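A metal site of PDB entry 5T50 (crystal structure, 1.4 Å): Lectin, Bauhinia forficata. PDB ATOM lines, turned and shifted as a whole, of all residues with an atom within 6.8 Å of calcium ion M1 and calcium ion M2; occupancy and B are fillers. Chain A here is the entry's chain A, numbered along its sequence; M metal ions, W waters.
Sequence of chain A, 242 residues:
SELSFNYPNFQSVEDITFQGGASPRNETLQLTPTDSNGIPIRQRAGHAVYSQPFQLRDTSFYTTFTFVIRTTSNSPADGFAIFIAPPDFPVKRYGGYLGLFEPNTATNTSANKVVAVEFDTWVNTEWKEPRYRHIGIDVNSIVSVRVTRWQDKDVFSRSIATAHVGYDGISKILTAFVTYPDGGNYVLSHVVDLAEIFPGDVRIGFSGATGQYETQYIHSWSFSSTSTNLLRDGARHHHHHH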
ATOM      1  N   ASP A  78     -28.551  -6.354  25.186  1.00  0.00           N
ATOM      2  CA  ASP A  78     -28.370  -5.937  23.786  1.00  0.00           C
ATOM      3  C   ASP A  78     -28.832  -4.522  23.457  1.00  0.00           C
ATOM      4  O   ASP A  78     -28.457  -3.981  22.424  1.00  0.00           O
ATOM      5  CB  ASP A  78     -29.154  -6.900  22.888  1.00  0.00           C
ATOM      6  CG  ASP A  78     -28.341  -8.106  22.556  1.00  0.00           C
ATOM      7  OD1 ASP A  78     -27.537  -8.032  21.620  1.00  0.00           O
ATOM      8  OD2 ASP A  78     -28.467  -9.111  23.318  1.00  0.00           O
ATOM      9  N   GLY A  95     -31.859 -11.247  22.395  1.00  0.00           N
ATOM     10  CA  GLY A  95     -30.551 -10.919  21.881  1.00  0.00           C
ATOM     11  C   GLY A  95     -30.519  -9.743  20.924  1.00  0.00           C
ATOM     12  O   GLY A  95     -31.323  -8.789  21.081  1.00  0.00           O
ATOM     13  N   GLY A  96     -29.716  -9.826  19.855  1.00  0.00           N
ATOM     14  CA  GLY A  96     -29.508  -8.664  18.977  1.00  0.00           C
ATOM     15  C   GLY A  96     -30.716  -8.301  18.136  1.00  0.00           C
ATOM     16  O   GLY A  96     -30.776  -7.210  17.540  1.00  0.00           O
ATOM     17  N   TYR A  97     -31.741  -9.192  18.074  1.00  0.00           N
ATOM     18  CA  TYR A  97     -32.987  -8.871  17.423  1.00  0.00           C
ATOM     19  C   TYR A  97     -33.825  -7.853  18.178  1.00  0.00           C
ATOM     20  O   TYR A  97     -34.851  -7.403  17.635  1.00  0.00           O
ATOM     21  CB  TYR A  97     -33.758 -10.151  17.151  1.00  0.00           C
ATOM     22  CG  TYR A  97     -32.997 -11.106  16.272  1.00  0.00           C
ATOM     23  CD1 TYR A  97     -32.859 -10.918  14.928  1.00  0.00           C
ATOM     24  CD2 TYR A  97     -32.330 -12.210  16.846  1.00  0.00           C
ATOM     25  CE1 TYR A  97     -32.083 -11.819  14.158  1.00  0.00           C
ATOM     26  CE2 TYR A  97     -31.560 -13.091  16.085  1.00  0.00           C
ATOM     27  CZ  TYR A  97     -31.445 -12.868  14.716  1.00  0.00           C
ATOM     28  OH  TYR A  97     -30.691 -13.775  13.948  1.00  0.00           O
ATOM     29  N   LEU A  98     -33.451  -7.576  19.446  1.00  0.00           N
ATOM     30  CA  LEU A  98     -34.066  -6.499  20.235  1.00  0.00           C
ATOM     31  C   LEU A  98     -35.527  -6.654  20.523  1.00  0.00           C
ATOM     32  O   LEU A  98     -36.236  -5.736  20.866  1.00  0.00           O
ATOM     33  CB  LEU A  98     -33.728  -5.111  19.637  1.00  0.00           C
ATOM     34  CG  LEU A  98     -32.284  -4.670  19.552  1.00  0.00           C
ATOM     35  CD1 LEU A  98     -32.168  -3.335  18.845  1.00  0.00           C
ATOM     36  CD2 LEU A  98     -31.739  -4.534  20.979  1.00  0.00           C
ATOM     37  N   GLU A 118     -33.486   2.696  17.886  1.00  0.00           N
ATOM     38  CA  GLU A 118     -32.801   1.722  18.709  1.00  0.00           C
ATOM     39  C   GLU A 118     -31.571   2.314  19.410  1.00  0.00           C
ATOM     40  O   GLU A 118     -30.899   3.213  18.875  1.00  0.00           O
ATOM     41  CB  GLU A 118     -32.354   0.479  17.908  1.00  0.00           C
ATOM     42  CG  GLU A 118     -31.361   0.785  16.798  1.00  0.00           C
ATOM     43  CD  GLU A 118     -30.718  -0.503  16.289  1.00  0.00           C
ATOM     44  OE1 GLU A 118     -31.543  -1.411  15.845  1.00  0.00           O
ATOM     45  OE2 GLU A 118     -29.454  -0.563  16.217  1.00  0.00           O
ATOM     46  N   ASP A 120     -28.351   0.644  20.851  1.00  0.00           N
ATOM     47  CA  ASP A 120     -27.762  -0.696  20.598  1.00  0.00           C
ATOM     48  C   ASP A 120     -26.432  -0.777  21.345  1.00  0.00           C
ATOM     49  O   ASP A 120     -25.455  -0.112  20.967  1.00  0.00           O
ATOM     50  CB  ASP A 120     -27.615  -0.928  19.116  1.00  0.00           C
ATOM     51  CG  ASP A 120     -27.254  -2.380  18.797  1.00  0.00           C
ATOM     52  OD1 ASP A 120     -26.742  -3.073  19.667  1.00  0.00           O
ATOM     53  OD2 ASP A 120     -27.515  -2.807  17.629  1.00  0.00           O
ATOM     54  N   THR A 121     -26.404  -1.591  22.409  1.00  0.00           N
ATOM     55  CA  THR A 121     -25.178  -1.741  23.226  1.00  0.00           C
ATOM     56  C   THR A 121     -24.218  -2.817  22.841  1.00  0.00           C
ATOM     57  O   THR A 121     -23.156  -2.930  23.453  1.00  0.00           O
ATOM     58  CB  THR A 121     -25.582  -1.988  24.735  1.00  0.00           C
ATOM     59  OG1 THR A 121     -26.324  -3.209  24.748  1.00  0.00           O
ATOM     60  CG2 THR A 121     -26.395  -0.847  25.294  1.00  0.00           C
ATOM     61  N   TRP A 122     -24.586  -3.621  21.834  1.00  0.00           N
ATOM     62  CA  TRP A 122     -23.823  -4.831  21.511  1.00  0.00           C
ATOM     63  C   TRP A 122     -23.650  -4.946  19.996  1.00  0.00           C
ATOM     64  O   TRP A 122     -24.586  -4.995  19.221  1.00  0.00           O
ATOM     65  CB  TRP A 122     -24.539  -6.074  22.030  1.00  0.00           C
ATOM     66  CG  TRP A 122     -23.846  -7.348  21.628  1.00  0.00           C
ATOM     67  CD1 TRP A 122     -24.062  -8.019  20.502  1.00  0.00           C
ATOM     68  CD2 TRP A 122     -22.823  -8.038  22.346  1.00  0.00           C
ATOM     69  NE1 TRP A 122     -23.262  -9.153  20.446  1.00  0.00           N
ATOM     70  CE2 TRP A 122     -22.453  -9.174  21.562  1.00  0.00           C
ATOM     71  CE3 TRP A 122     -22.197  -7.859  23.585  1.00  0.00           C
ATOM     72  CZ2 TRP A 122     -21.501 -10.101  21.995  1.00  0.00           C
ATOM     73  CZ3 TRP A 122     -21.262  -8.749  24.016  1.00  0.00           C
ATOM     74  CH2 TRP A 122     -20.931  -9.888  23.205  1.00  0.00           C
ATOM     75  N   VAL A 123     -22.399  -4.944  19.566  1.00  0.00           N
ATOM     76  CA  VAL A 123     -22.072  -5.020  18.146  1.00  0.00           C
ATOM     77  C   VAL A 123     -22.269  -6.470  17.680  1.00  0.00           C
ATOM     78  O   VAL A 123     -21.570  -7.393  18.102  1.00  0.00           O
ATOM     79  CB  VAL A 123     -20.610  -4.560  17.888  1.00  0.00           C
ATOM     80  CG1 VAL A 123     -20.224  -4.892  16.447  1.00  0.00           C
ATOM     81  CG2 VAL A 123     -20.420  -3.090  18.275  1.00  0.00           C
ATOM     82  N   ASN A 124     -23.243  -6.623  16.770  1.00  0.00           N
ATOM     83  CA  ASN A 124     -23.563  -7.943  16.175  1.00  0.00           C
ATOM     84  C   ASN A 124     -22.755  -8.157  14.904  1.00  0.00           C
ATOM     85  O   ASN A 124     -22.680  -7.211  14.096  1.00  0.00           O
ATOM     86  CB  ASN A 124     -25.036  -8.059  15.884  1.00  0.00           C
ATOM     87  CG  ASN A 124     -25.811  -8.268  17.188  1.00  0.00           C
ATOM     88  OD1 ASN A 124     -26.321  -7.334  17.805  1.00  0.00           O
ATOM     89  ND2 ASN A 124     -25.831  -9.537  17.637  1.00  0.00           N
ATOM     90  N   TRP A 127     -25.304  -9.598  11.131  1.00  0.00           N
ATOM     91  CA  TRP A 127     -25.801  -8.696  10.103  1.00  0.00           C
ATOM     92  C   TRP A 127     -24.882  -7.488  10.136  1.00  0.00           C
ATOM     93  O   TRP A 127     -24.087  -7.356  11.087  1.00  0.00           O
ATOM     94  CB  TRP A 127     -27.253  -8.297  10.338  1.00  0.00           C
ATOM     95  CG  TRP A 127     -27.551  -7.820  11.690  1.00  0.00           C
ATOM     96  CD1 TRP A 127     -27.420  -6.516  12.207  1.00  0.00           C
ATOM     97  CD2 TRP A 127     -28.056  -8.602  12.771  1.00  0.00           C
ATOM     98  NE1 TRP A 127     -27.746  -6.541  13.517  1.00  0.00           N
ATOM     99  CE2 TRP A 127     -28.128  -7.781  13.922  1.00  0.00           C
ATOM    100  CE3 TRP A 127     -28.375  -9.949  12.906  1.00  0.00           C
ATOM    101  CZ2 TRP A 127     -28.616  -8.255  15.130  1.00  0.00           C
ATOM    102  CZ3 TRP A 127     -28.792 -10.418  14.146  1.00  0.00           C
ATOM    103  CH2 TRP A 127     -28.906  -9.567  15.242  1.00  0.00           C
ATOM    104  N   LYS A 128     -25.109  -6.552   9.210  1.00  0.00           N
ATOM    105  CA  LYS A 128     -24.271  -5.356   9.177  1.00  0.00           C
ATOM    106  C   LYS A 128     -24.670  -4.303  10.164  1.00  0.00           C
ATOM    107  O   LYS A 128     -25.830  -3.859  10.145  1.00  0.00           O
ATOM    108  CB  LYS A 128     -24.369  -4.725   7.805  1.00  0.00           C
ATOM    109  CG  LYS A 128     -23.640  -5.554   6.787  1.00  0.00           C
ATOM    110  CD  LYS A 128     -22.145  -5.272   6.690  1.00  0.00           C
ATOM    111  CE  LYS A 128     -21.532  -5.999   5.498  1.00  0.00           C
ATOM    112  NZ  LYS A 128     -20.100  -6.367   5.768  1.00  0.00           N
ATOM    113  N   GLU A 129     -23.765  -4.000  11.065  1.00  0.00           N
ATOM    114  CA  GLU A 129     -23.888  -2.803  11.889  1.00  0.00           C
ATOM    115  C   GLU A 129     -22.543  -2.249  12.251  1.00  0.00           C
ATOM    116  O   GLU A 129     -21.523  -2.883  12.019  1.00  0.00           O
ATOM    117  CB  GLU A 129     -24.812  -3.040  13.036  1.00  0.00           C
ATOM    118  CG  GLU A 129     -24.408  -4.054  14.036  1.00  0.00           C
ATOM    119  CD  GLU A 129     -25.544  -4.251  15.112  1.00  0.00           C
ATOM    120  OE1 GLU A 129     -26.779  -3.909  14.888  1.00  0.00           O
ATOM    121  OE2 GLU A 129     -25.156  -4.670  16.224  1.00  0.00           O
ATOM    122  N   PRO A 130     -22.530  -0.988  12.774  1.00  0.00           N
ATOM    123  CA  PRO A 130     -21.245  -0.405  13.094  1.00  0.00           C
ATOM    124  C   PRO A 130     -20.434  -1.174  14.111  1.00  0.00           C
ATOM    125  O   PRO A 130     -21.001  -1.920  14.899  1.00  0.00           O
ATOM    126  CB  PRO A 130     -21.652   0.958  13.673  1.00  0.00           C
ATOM    127  CG  PRO A 130     -23.010   1.230  13.212  1.00  0.00           C
ATOM    128  CD  PRO A 130     -23.655  -0.092  13.007  1.00  0.00           C
ATOM    129  N   HIS A 134     -24.168   2.153  19.190  1.00  0.00           N
ATOM    130  CA  HIS A 134     -24.821   3.092  18.267  1.00  0.00           C
ATOM    131  C   HIS A 134     -26.288   3.258  18.549  1.00  0.00           C
ATOM    132  O   HIS A 134     -26.921   2.405  19.172  1.00  0.00           O
ATOM    133  CB  HIS A 134     -24.592   2.629  16.802  1.00  0.00           C
ATOM    134  CG  HIS A 134     -25.016   1.221  16.525  1.00  0.00           C
ATOM    135  ND1 HIS A 134     -24.186   0.168  16.786  1.00  0.00           N
ATOM    136  CD2 HIS A 134     -26.174   0.695  16.069  1.00  0.00           C
ATOM    137  CE1 HIS A 134     -24.825  -0.940  16.504  1.00  0.00           C
ATOM    138  NE2 HIS A 134     -26.002  -0.657  16.055  1.00  0.00           N
ATOM    139  N   GLY A 136     -29.765   4.164  16.305  1.00  0.00           N
ATOM    140  CA  GLY A 136     -30.200   4.037  14.936  1.00  0.00           C
ATOM    141  C   GLY A 136     -31.657   4.186  14.711  1.00  0.00           C
ATOM    142  O   GLY A 136     -32.457   3.998  15.631  1.00  0.00           O
ATOM    143  N   ASP A 138     -34.522   2.315  12.505  1.00  0.00           N
ATOM    144  CA  ASP A 138     -34.758   1.058  11.841  1.00  0.00           C
ATOM    145  C   ASP A 138     -36.098   1.160  11.128  1.00  0.00           C
ATOM    146  O   ASP A 138     -37.113   1.531  11.734  1.00  0.00           O
ATOM    147  CB  ASP A 138     -34.823  -0.091  12.861  1.00  0.00           C
ATOM    148  CG  ASP A 138     -33.584  -0.305  13.637  1.00  0.00           C
ATOM    149  OD1 ASP A 138     -32.540   0.180  13.234  1.00  0.00           O
ATOM    150  OD2 ASP A 138     -33.676  -0.949  14.722  1.00  0.00           O
ATOM    151  N   ILE A 142     -33.518  -4.988  10.961  1.00  0.00           N
ATOM    152  CA  ILE A 142     -32.540  -4.824  12.042  1.00  0.00           C
ATOM    153  C   ILE A 142     -31.274  -4.087  11.623  1.00  0.00           C
ATOM    154  O   ILE A 142     -30.505  -3.635  12.494  1.00  0.00           O
ATOM    155  CB  ILE A 142     -32.224  -6.202  12.672  1.00  0.00           C
ATOM    156  CG1 ILE A 142     -31.615  -6.131  14.091  1.00  0.00           C
ATOM    157  CG2 ILE A 142     -31.367  -7.042  11.668  1.00  0.00           C
ATOM    158  CD1 ILE A 142     -32.470  -5.347  15.127  1.00  0.00           C
ATOM    159  N   VAL A 143     -31.078  -3.911  10.305  1.00  0.00           N
ATOM    160  CA  VAL A 143     -29.957  -3.149   9.761  1.00  0.00           C
ATOM    161  C   VAL A 143     -30.476  -1.702   9.635  1.00  0.00           C
ATOM    162  O   VAL A 143     -31.315  -1.386   8.796  1.00  0.00           O
ATOM    163  CB  VAL A 143     -29.469  -3.729   8.425  1.00  0.00           C
ATOM    164  CG1 VAL A 143     -28.392  -2.809   7.835  1.00  0.00           C
ATOM    165  CG2 VAL A 143     -28.889  -5.106   8.589  1.00  0.00           C
ATOM    166  N   SER A 144     -29.984  -0.837  10.498  1.00  0.00           N
ATOM    167  CA  SER A 144     -30.446   0.532  10.548  1.00  0.00           C
ATOM    168  C   SER A 144     -30.222   1.274   9.244  1.00  0.00           C
ATOM    169  O   SER A 144     -29.159   1.193   8.652  1.00  0.00           O
ATOM    170  CB  SER A 144     -29.761   1.294  11.713  1.00  0.00           C
ATOM    171  OG  SER A 144     -29.961   0.671  12.975  1.00  0.00           O
ATOM    172  N   VAL A 147     -27.671   5.670  11.275  1.00  0.00           N
ATOM    173  CA  VAL A 147     -27.070   5.188  12.515  1.00  0.00           C
ATOM    174  C   VAL A 147     -25.961   6.147  12.866  1.00  0.00           C
ATOM    175  O   VAL A 147     -25.318   6.735  11.961  1.00  0.00           O
ATOM    176  CB  VAL A 147     -26.568   3.686  12.278  1.00  0.00           C
ATOM    177  CG1 VAL A 147     -25.380   3.619  11.322  1.00  0.00           C
ATOM    178  CG2 VAL A 147     -26.359   2.948  13.525  1.00  0.00           C
HETATM  179 CA    CA M   1     -27.941  -2.080  15.560  1.00  0.00          CA
HETATM  180 CA    CA M   2     -26.661  -5.034  18.149  1.00  0.00          CA
HETATM  181  O   HOH W   1     -29.831  -3.413  15.171  1.00  0.00           O
HETATM  182  O   HOH W   2     -27.734  -5.732  20.161  1.00  0.00           O
HETATM  183  O   HOH W   3     -28.819  -5.389  17.093  1.00  0.00           O
HETATM  184  O   HOH W   4     -27.970  -1.011  13.541  1.00  0.00           O
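Calcium ion M1 is bound by OD2 of Asp 120 (2.2 Å), OE2 of Glu 118 (2.2 Å), OE1 of Glu 129 (2.3 Å), water W4 (2.3 Å), water W1 (2.3 Å) and NE2 of His 134 (2.5 Å).
Calcium ion M1 has six donor atoms within binding distance.
Calcium ion M2 is bound by the backbone carbonyl oxygen (O) of Trp 122, 2.3 Å away.
OD1 of Asn 124 binds calcium ion M2 (2.4 Å).
Water W2 is bound to calcium ion M2 (2.4 Å).
Calcium ion M2 is bound by water W3.
Calcium ion M2 is bound by the side-chain carboxylate (OD2) of Asp 120 (2.4 Å).
The side-chain carboxylate (OE2) of Glu 129 binds calcium ion M2 (2.5 Å).
OD1 of Asp 120 binds calcium ion M2 (2.5 Å).
Calcium ion M2 has seven donor atoms within binding distance.
Water W1 lies within hydrogen-bond range of the side-chain carboxylate (OE1) of Glu 118 and the backbone carbonyl oxygen (O) of Ile 142.
Four residues have an atom within 4 Å of calcium ion M1: Glu 118, Asp 120, Glu 129 and His 134.
Along chain A the residues within 4 Å of calcium ion M1 span positions 118 to 134.
The nearest printed residue that does not touch calcium ion M1 is Ser 144 (4.3 Å).
Four residues have an atom within 4 Å of calcium ion M2: Asp 120, Trp 122, Asn 124 and Glu 129.
The nearest printed residue that does not touch calcium ion M2 is Val 123 (4.5 Å).
OE1 of Glu 118 sits close to OD2 of Asp 138, at 2.5 Å.
N of Glu 118 sits at hydrogen-bond distance from O of Gly 136, at 2.8 Å.
NE1 of Trp 127 lies close to OE1 of Glu 129 (3.1 Å).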
